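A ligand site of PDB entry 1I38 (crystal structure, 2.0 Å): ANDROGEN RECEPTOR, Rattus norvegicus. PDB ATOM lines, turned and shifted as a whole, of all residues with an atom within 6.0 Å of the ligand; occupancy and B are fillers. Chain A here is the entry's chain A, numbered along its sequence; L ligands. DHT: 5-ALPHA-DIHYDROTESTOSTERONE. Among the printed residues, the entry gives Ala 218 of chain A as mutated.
An oxygen (O3) of the ligand sits at hydrogen-bond distance from the guanidinium group of Arg 93 (3.0 Å).
An oxygen (O17) of the ligand lies within hydrogen-bond range of the side-chain amide nitrogen (ND2) of Asn 46 (3.0 Å).
O3 of the ligand lies close to OE1 of Gln 52 (3.3 Å).
NH2 of Arg 93 is in hydrogen-bond range of O of Phe 105 (2.8 Å).
NE of Arg 93 lies within hydrogen-bond range of O of Tyr 104 (3.1 Å).
OD1 of Asn 46 sits close to O of Leu 42 (3.3 Å).
CD1 of Leu 42 touches C17 of the ligand, at 3.9 Å.
O of Leu 45 touches C11 of the ligand, at 3.5 Å.
CD2 of Leu 48 touches C2 of the ligand (3.7 Å).
Gly 49 touches the ligand (CA to C1, 3.9 Å).
Trp 82 touches the ligand.
Met 83 touches the ligand.
Met 86 touches the ligand.
Met 90 touches the ligand (CB to O3, 3.8 Å).
CD2 of Phe 105 touches C4 of the ligand, 3.5 Å away.
Met 128 touches the ligand.
Phe 217 touches the ligand.
CB of Ala 218 touches C18 of the ligand, at 3.4 Å.
CD2 of Leu 221 touches O17 of the ligand, at 3.8 Å.
Phe 232 touches the ligand (CE2 to O17, 3.7 Å).
Met 236 touches the ligand.
Of the 25 residues printed, 18 come within 4 Å of the ligand.
Along chain A the residues within 4 Å of the ligand span positions 42 to 236.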
ATOM      1  N   LEU A  42      12.295   9.547  -0.019  1.00  0.00           N
ATOM      2  CA  LEU A  42      12.911  10.864   0.020  1.00  0.00           C
ATOM      3  C   LEU A  42      12.632  11.717  -1.229  1.00  0.00           C
ATOM      4  O   LEU A  42      12.585  12.960  -1.162  1.00  0.00           O
ATOM      5  CB  LEU A  42      14.410  10.724   0.280  1.00  0.00           C
ATOM      6  CG  LEU A  42      14.799  10.627   1.763  1.00  0.00           C
ATOM      7  CD1 LEU A  42      14.383  11.921   2.473  1.00  0.00           C
ATOM      8  CD2 LEU A  42      14.120   9.439   2.420  1.00  0.00           C
ATOM      9  N   LEU A  45       9.149  12.918  -0.664  1.00  0.00           N
ATOM     10  CA  LEU A  45       9.178  13.953   0.349  1.00  0.00           C
ATOM     11  C   LEU A  45       9.704  15.237  -0.288  1.00  0.00           C
ATOM     12  O   LEU A  45       9.140  16.317  -0.069  1.00  0.00           O
ATOM     13  CB  LEU A  45      10.079  13.531   1.517  1.00  0.00           C
ATOM     14  CG  LEU A  45       9.464  12.504   2.469  1.00  0.00           C
ATOM     15  CD1 LEU A  45      10.497  12.064   3.499  1.00  0.00           C
ATOM     16  CD2 LEU A  45       8.216  13.088   3.145  1.00  0.00           C
ATOM     17  N   ASN A  46      10.775  15.118  -1.076  1.00  0.00           N
ATOM     18  CA  ASN A  46      11.375  16.256  -1.768  1.00  0.00           C
ATOM     19  C   ASN A  46      10.341  16.920  -2.666  1.00  0.00           C
ATOM     20  O   ASN A  46      10.180  18.150  -2.623  1.00  0.00           O
ATOM     21  CB  ASN A  46      12.571  15.806  -2.623  1.00  0.00           C
ATOM     22  CG  ASN A  46      13.832  15.551  -1.801  1.00  0.00           C
ATOM     23  OD1 ASN A  46      14.824  15.021  -2.323  1.00  0.00           O
ATOM     24  ND2 ASN A  46      13.809  15.923  -0.543  1.00  0.00           N
ATOM     25  N   LEU A  48       7.169  16.670  -2.450  1.00  0.00           N
ATOM     26  CA  LEU A  48       6.159  17.217  -1.557  1.00  0.00           C
ATOM     27  C   LEU A  48       6.694  18.550  -1.082  1.00  0.00           C
ATOM     28  O   LEU A  48       5.936  19.507  -0.935  1.00  0.00           O
ATOM     29  CB  LEU A  48       5.908  16.287  -0.366  1.00  0.00           C
ATOM     30  CG  LEU A  48       4.962  16.855   0.694  1.00  0.00           C
ATOM     31  CD1 LEU A  48       3.570  17.116   0.104  1.00  0.00           C
ATOM     32  CD2 LEU A  48       4.873  15.900   1.860  1.00  0.00           C
ATOM     33  N   GLY A  49       8.007  18.615  -0.882  1.00  0.00           N
ATOM     34  CA  GLY A  49       8.619  19.850  -0.429  1.00  0.00           C
ATOM     35  C   GLY A  49       8.431  20.994  -1.400  1.00  0.00           C
ATOM     36  O   GLY A  49       8.070  22.101  -1.004  1.00  0.00           O
ATOM     37  N   GLN A  52       4.652  22.089  -1.346  1.00  0.00           N
ATOM     38  CA  GLN A  52       4.189  22.865  -0.207  1.00  0.00           C
ATOM     39  C   GLN A  52       4.862  24.228  -0.139  1.00  0.00           C
ATOM     40  O   GLN A  52       4.286  25.188   0.376  1.00  0.00           O
ATOM     41  CB  GLN A  52       4.387  22.088   1.092  1.00  0.00           C
ATOM     42  CG  GLN A  52       3.169  21.252   1.451  1.00  0.00           C
ATOM     43  CD  GLN A  52       3.422  20.303   2.595  1.00  0.00           C
ATOM     44  OE1 GLN A  52       3.914  20.699   3.654  1.00  0.00           O
ATOM     45  NE2 GLN A  52       3.084  19.040   2.390  1.00  0.00           N
ATOM     46  N   TRP A  82      10.562  27.910   6.347  1.00  0.00           N
ATOM     47  CA  TRP A  82       9.854  26.799   5.712  1.00  0.00           C
ATOM     48  C   TRP A  82       9.966  25.407   6.350  1.00  0.00           C
ATOM     49  O   TRP A  82       9.003  24.652   6.349  1.00  0.00           O
ATOM     50  CB  TRP A  82      10.229  26.687   4.223  1.00  0.00           C
ATOM     51  CG  TRP A  82      11.613  26.212   3.988  1.00  0.00           C
ATOM     52  CD1 TRP A  82      12.754  26.946   4.094  1.00  0.00           C
ATOM     53  CD2 TRP A  82      12.025  24.867   3.683  1.00  0.00           C
ATOM     54  NE1 TRP A  82      13.856  26.144   3.868  1.00  0.00           N
ATOM     55  CE2 TRP A  82      13.431  24.865   3.616  1.00  0.00           C
ATOM     56  CE3 TRP A  82      11.334  23.669   3.458  1.00  0.00           C
ATOM     57  CZ2 TRP A  82      14.164  23.711   3.342  1.00  0.00           C
ATOM     58  CZ3 TRP A  82      12.067  22.514   3.183  1.00  0.00           C
ATOM     59  CH2 TRP A  82      13.468  22.543   3.126  1.00  0.00           C
ATOM     60  N   MET A  83      11.133  25.039   6.878  1.00  0.00           N
ATOM     61  CA  MET A  83      11.207  23.702   7.475  1.00  0.00           C
ATOM     62  C   MET A  83      10.319  23.669   8.711  1.00  0.00           C
ATOM     63  O   MET A  83       9.517  22.757   8.869  1.00  0.00           O
ATOM     64  CB  MET A  83      12.646  23.347   7.857  1.00  0.00           C
ATOM     65  CG  MET A  83      12.803  21.906   8.371  1.00  0.00           C
ATOM     66  SD  MET A  83      12.474  20.677   7.104  1.00  0.00           S
ATOM     67  CE  MET A  83      14.048  20.647   6.220  1.00  0.00           C
ATOM     68  N   MET A  86       6.436  23.793   7.805  1.00  0.00           N
ATOM     69  CA  MET A  86       5.928  22.541   7.277  1.00  0.00           C
ATOM     70  C   MET A  86       5.834  21.388   8.279  1.00  0.00           C
ATOM     71  O   MET A  86       4.870  20.617   8.235  1.00  0.00           O
ATOM     72  CB  MET A  86       6.747  22.102   6.069  1.00  0.00           C
ATOM     73  CG  MET A  86       6.622  23.036   4.880  1.00  0.00           C
ATOM     74  SD  MET A  86       7.684  22.493   3.521  1.00  0.00           S
ATOM     75  CE  MET A  86       7.477  23.888   2.364  1.00  0.00           C
ATOM     76  N   VAL A  87       6.820  21.263   9.168  1.00  0.00           N
ATOM     77  CA  VAL A  87       6.792  20.196  10.171  1.00  0.00           C
ATOM     78  C   VAL A  87       5.630  20.424  11.113  1.00  0.00           C
ATOM     79  O   VAL A  87       4.904  19.488  11.429  1.00  0.00           O
ATOM     80  CB  VAL A  87       8.085  20.150  10.999  1.00  0.00           C
ATOM     81  CG1 VAL A  87       7.930  19.162  12.143  1.00  0.00           C
ATOM     82  CG2 VAL A  87       9.245  19.710  10.133  1.00  0.00           C
ATOM     83  N   MET A  90       2.493  19.607   9.419  1.00  0.00           N
ATOM     84  CA  MET A  90       2.454  18.168   9.247  1.00  0.00           C
ATOM     85  C   MET A  90       2.119  17.522  10.579  1.00  0.00           C
ATOM     86  O   MET A  90       1.314  16.588  10.651  1.00  0.00           O
ATOM     87  CB  MET A  90       3.795  17.660   8.727  1.00  0.00           C
ATOM     88  CG  MET A  90       3.811  16.195   8.383  1.00  0.00           C
ATOM     89  SD  MET A  90       3.865  15.125   9.839  1.00  0.00           S
ATOM     90  CE  MET A  90       5.626  14.959  10.062  1.00  0.00           C
ATOM     91  N   ARG A  93      -1.532  17.788  10.875  1.00  0.00           N
ATOM     92  CA  ARG A  93      -2.345  16.931  10.018  1.00  0.00           C
ATOM     93  C   ARG A  93      -2.391  15.555  10.660  1.00  0.00           C
ATOM     94  O   ARG A  93      -3.420  14.871  10.621  1.00  0.00           O
ATOM     95  CB  ARG A  93      -1.759  16.813   8.613  1.00  0.00           C
ATOM     96  CG  ARG A  93      -1.935  18.056   7.763  1.00  0.00           C
ATOM     97  CD  ARG A  93      -1.611  17.769   6.294  1.00  0.00           C
ATOM     98  NE  ARG A  93      -0.204  17.486   6.041  1.00  0.00           N
ATOM     99  CZ  ARG A  93       0.764  18.403   6.059  1.00  0.00           C
ATOM    100  NH1 ARG A  93       0.476  19.673   6.315  1.00  0.00           N
ATOM    101  NH2 ARG A  93       2.011  18.057   5.787  1.00  0.00           N
ATOM    102  N   TYR A 104       1.474  12.162   9.055  1.00  0.00           N
ATOM    103  CA  TYR A 104       0.654  12.534   7.900  1.00  0.00           C
ATOM    104  C   TYR A 104       1.292  13.629   7.040  1.00  0.00           C
ATOM    105  O   TYR A 104       0.918  14.810   7.142  1.00  0.00           O
ATOM    106  CB  TYR A 104      -0.728  13.014   8.386  1.00  0.00           C
ATOM    107  CG  TYR A 104      -1.825  12.817   7.370  1.00  0.00           C
ATOM    108  CD1 TYR A 104      -2.452  11.585   7.225  1.00  0.00           C
ATOM    109  CD2 TYR A 104      -2.199  13.860   6.506  1.00  0.00           C
ATOM    110  CE1 TYR A 104      -3.414  11.373   6.249  1.00  0.00           C
ATOM    111  CE2 TYR A 104      -3.169  13.660   5.528  1.00  0.00           C
ATOM    112  CZ  TYR A 104      -3.776  12.410   5.410  1.00  0.00           C
ATOM    113  OH  TYR A 104      -4.752  12.187   4.470  1.00  0.00           O
ATOM    114  N   PHE A 105       2.242  13.235   6.196  1.00  0.00           N
ATOM    115  CA  PHE A 105       2.893  14.194   5.315  1.00  0.00           C
ATOM    116  C   PHE A 105       1.893  14.677   4.286  1.00  0.00           C
ATOM    117  O   PHE A 105       1.728  15.884   4.066  1.00  0.00           O
ATOM    118  CB  PHE A 105       4.080  13.545   4.608  1.00  0.00           C
ATOM    119  CG  PHE A 105       5.242  13.253   5.514  1.00  0.00           C
ATOM    120  CD1 PHE A 105       5.553  11.936   5.869  1.00  0.00           C
ATOM    121  CD2 PHE A 105       6.027  14.289   6.003  1.00  0.00           C
ATOM    122  CE1 PHE A 105       6.638  11.661   6.690  1.00  0.00           C
ATOM    123  CE2 PHE A 105       7.105  14.025   6.821  1.00  0.00           C
ATOM    124  CZ  PHE A 105       7.410  12.712   7.165  1.00  0.00           C
ATOM    125  N   ALA A 106       1.235  13.719   3.650  1.00  0.00           N
ATOM    126  CA  ALA A 106       0.235  14.015   2.637  1.00  0.00           C
ATOM    127  C   ALA A 106      -0.717  12.826   2.615  1.00  0.00           C
ATOM    128  O   ALA A 106      -0.394  11.776   3.171  1.00  0.00           O
ATOM    129  CB  ALA A 106       0.909  14.203   1.278  1.00  0.00           C
ATOM    130  N   MET A 121      15.366   7.938   8.402  1.00  0.00           N
ATOM    131  CA  MET A 121      15.025   9.140   9.141  1.00  0.00           C
ATOM    132  C   MET A 121      14.340   8.825  10.461  1.00  0.00           C
ATOM    133  O   MET A 121      13.544   9.630  10.967  1.00  0.00           O
ATOM    134  CB  MET A 121      14.110  10.019   8.287  1.00  0.00           C
ATOM    135  CG  MET A 121      14.734  11.306   7.795  1.00  0.00           C
ATOM    136  SD  MET A 121      13.645  12.085   6.602  1.00  0.00           S
ATOM    137  CE  MET A 121      12.238  12.505   7.633  1.00  0.00           C
ATOM    138  N   MET A 128       9.007  14.286  15.482  1.00  0.00           N
ATOM    139  CA  MET A 128       7.831  14.864  14.842  1.00  0.00           C
ATOM    140  C   MET A 128       6.532  14.192  15.296  1.00  0.00           C
ATOM    141  O   MET A 128       5.495  14.851  15.464  1.00  0.00           O
ATOM    142  CB  MET A 128       7.970  14.759  13.323  1.00  0.00           C
ATOM    143  CG  MET A 128       9.199  15.464  12.807  1.00  0.00           C
ATOM    144  SD  MET A 128       9.525  15.150  11.088  1.00  0.00           S
ATOM    145  CE  MET A 128       8.656  16.425  10.395  1.00  0.00           C
ATOM    146  N   LEU A 214      16.417  18.211  10.610  1.00  0.00           N
ATOM    147  CA  LEU A 214      15.974  17.989   9.246  1.00  0.00           C
ATOM    148  C   LEU A 214      16.840  18.832   8.301  1.00  0.00           C
ATOM    149  O   LEU A 214      17.198  18.384   7.225  1.00  0.00           O
ATOM    150  CB  LEU A 214      14.480  18.318   9.140  1.00  0.00           C
ATOM    151  CG  LEU A 214      13.611  17.389  10.019  1.00  0.00           C
ATOM    152  CD1 LEU A 214      12.188  17.878  10.107  1.00  0.00           C
ATOM    153  CD2 LEU A 214      13.641  15.975   9.451  1.00  0.00           C
ATOM    154  N   PHE A 217      20.022  17.087   7.796  1.00  0.00           N
ATOM    155  CA  PHE A 217      19.715  15.885   7.028  1.00  0.00           C
ATOM    156  C   PHE A 217      19.460  16.168   5.549  1.00  0.00           C
ATOM    157  O   PHE A 217      20.024  15.496   4.674  1.00  0.00           O
ATOM    158  CB  PHE A 217      18.517  15.183   7.658  1.00  0.00           C
ATOM    159  CG  PHE A 217      18.317  13.784   7.156  1.00  0.00           C
ATOM    160  CD1 PHE A 217      17.740  13.551   5.909  1.00  0.00           C
ATOM    161  CD2 PHE A 217      18.691  12.698   7.946  1.00  0.00           C
ATOM    162  CE1 PHE A 217      17.543  12.260   5.454  1.00  0.00           C
ATOM    163  CE2 PHE A 217      18.492  11.397   7.489  1.00  0.00           C
ATOM    164  CZ  PHE A 217      17.918  11.174   6.243  1.00  0.00           C
ATOM    165  N   ALA A 218      18.617  17.147   5.273  1.00  0.00           N
ATOM    166  CA  ALA A 218      18.321  17.502   3.889  1.00  0.00           C
ATOM    167  C   ALA A 218      19.608  17.873   3.171  1.00  0.00           C
ATOM    168  O   ALA A 218      19.808  17.510   2.018  1.00  0.00           O
ATOM    169  CB  ALA A 218      17.344  18.674   3.840  1.00  0.00           C
ATOM    170  N   PHE A 219      20.466  18.602   3.870  1.00  0.00           N
ATOM    171  CA  PHE A 219      21.745  19.060   3.330  1.00  0.00           C
ATOM    172  C   PHE A 219      22.679  17.935   2.908  1.00  0.00           C
ATOM    173  O   PHE A 219      23.180  17.932   1.784  1.00  0.00           O
ATOM    174  CB  PHE A 219      22.463  19.953   4.359  1.00  0.00           C
ATOM    175  CG  PHE A 219      23.847  20.364   3.933  1.00  0.00           C
ATOM    176  CD1 PHE A 219      24.034  21.338   2.964  1.00  0.00           C
ATOM    177  CD2 PHE A 219      24.963  19.766   4.501  1.00  0.00           C
ATOM    178  CE1 PHE A 219      25.315  21.709   2.558  1.00  0.00           C
ATOM    179  CE2 PHE A 219      26.254  20.135   4.098  1.00  0.00           C
ATOM    180  CZ  PHE A 219      26.419  21.104   3.123  1.00  0.00           C
ATOM    181  N   LEU A 221      21.959  14.849   2.332  1.00  0.00           N
ATOM    182  CA  LEU A 221      21.292  14.100   1.293  1.00  0.00           C
ATOM    183  C   LEU A 221      21.487  14.760  -0.060  1.00  0.00           C
ATOM    184  O   LEU A 221      21.717  14.084  -1.046  1.00  0.00           O
ATOM    185  CB  LEU A 221      19.797  14.004   1.612  1.00  0.00           C
ATOM    186  CG  LEU A 221      18.938  13.178   0.647  1.00  0.00           C
ATOM    187  CD1 LEU A 221      19.525  11.786   0.509  1.00  0.00           C
ATOM    188  CD2 LEU A 221      17.517  13.106   1.177  1.00  0.00           C
ATOM    189  N   PHE A 232      16.129  15.792  -6.295  1.00  0.00           N
ATOM    190  CA  PHE A 232      15.767  17.024  -5.602  1.00  0.00           C
ATOM    191  C   PHE A 232      15.216  18.019  -6.605  1.00  0.00           C
ATOM    192  O   PHE A 232      15.915  18.414  -7.531  1.00  0.00           O
ATOM    193  CB  PHE A 232      16.992  17.659  -4.920  1.00  0.00           C
ATOM    194  CG  PHE A 232      17.265  17.162  -3.515  1.00  0.00           C
ATOM    195  CD1 PHE A 232      17.987  15.990  -3.293  1.00  0.00           C
ATOM    196  CD2 PHE A 232      16.831  17.884  -2.412  1.00  0.00           C
ATOM    197  CE1 PHE A 232      18.274  15.544  -1.997  1.00  0.00           C
ATOM    198  CE2 PHE A 232      17.110  17.459  -1.108  1.00  0.00           C
ATOM    199  CZ  PHE A 232      17.838  16.287  -0.904  1.00  0.00           C
ATOM    200  N   MET A 236      13.856  23.203  -4.124  1.00  0.00           N
ATOM    201  CA  MET A 236      14.463  22.541  -2.979  1.00  0.00           C
ATOM    202  C   MET A 236      15.991  22.498  -3.021  1.00  0.00           C
ATOM    203  O   MET A 236      16.640  22.707  -2.004  1.00  0.00           O
ATOM    204  CB  MET A 236      13.922  21.117  -2.853  1.00  0.00           C
ATOM    205  CG  MET A 236      12.455  21.052  -2.493  1.00  0.00           C
ATOM    206  SD  MET A 236      12.139  21.627  -0.826  1.00  0.00           S
ATOM    207  CE  MET A 236      12.093  20.161  -0.008  1.00  0.00           C
ATOM    208  N   ILE A 240      18.173  24.518  -0.105  1.00  0.00           N
ATOM    209  CA  ILE A 240      19.007  23.699   0.748  1.00  0.00           C
ATOM    210  C   ILE A 240      20.502  24.016   0.593  1.00  0.00           C
ATOM    211  O   ILE A 240      21.264  23.895   1.550  1.00  0.00           O
ATOM    212  CB  ILE A 240      18.749  22.186   0.487  1.00  0.00           C
ATOM    213  CG1 ILE A 240      17.317  21.851   0.890  1.00  0.00           C
ATOM    214  CG2 ILE A 240      19.754  21.344   1.286  1.00  0.00           C
ATOM    215  CD1 ILE A 240      16.897  20.401   0.687  1.00  0.00           C
HETATM  216  C1  DHT L   1       7.982  18.251   3.049  1.00  0.00           C
HETATM  217  C2  DHT L   1       6.576  18.779   3.519  1.00  0.00           C
HETATM  218  C3  DHT L   1       6.147  18.085   4.831  1.00  0.00           C
HETATM  219  O3  DHT L   1       4.952  17.938   5.072  1.00  0.00           O
HETATM  220  C4  DHT L   1       7.163  17.584   5.791  1.00  0.00           C
HETATM  221  C5  DHT L   1       8.473  17.735   5.564  1.00  0.00           C
HETATM  222  C6  DHT L   1       9.462  17.218   6.640  1.00  0.00           C
HETATM  223  C7  DHT L   1      10.674  16.418   6.040  1.00  0.00           C
HETATM  224  C8  DHT L   1      11.376  17.149   4.854  1.00  0.00           C
HETATM  225  C9  DHT L   1      10.316  17.378   3.726  1.00  0.00           C
HETATM  226  C10 DHT L   1       9.086  18.301   4.168  1.00  0.00           C
HETATM  227  C11 DHT L   1      10.989  17.923   2.400  1.00  0.00           C
HETATM  228  C12 DHT L   1      12.201  17.068   1.934  1.00  0.00           C
HETATM  229  C13 DHT L   1      13.294  16.925   3.064  1.00  0.00           C
HETATM  230  C14 DHT L   1      12.531  16.274   4.308  1.00  0.00           C
HETATM  231  C15 DHT L   1      13.709  15.910   5.279  1.00  0.00           C
HETATM  232  C16 DHT L   1      14.835  15.417   4.297  1.00  0.00           C
HETATM  233  C17 DHT L   1      14.364  15.799   2.839  1.00  0.00           C
HETATM  234  O17 DHT L   1      15.527  16.247   1.951  1.00  0.00           O
HETATM  235  C18 DHT L   1      14.017  18.302   3.378  1.00  0.00           C
HETATM  236  C19 DHT L   1       9.509  19.801   4.479  1.00  0.00           C
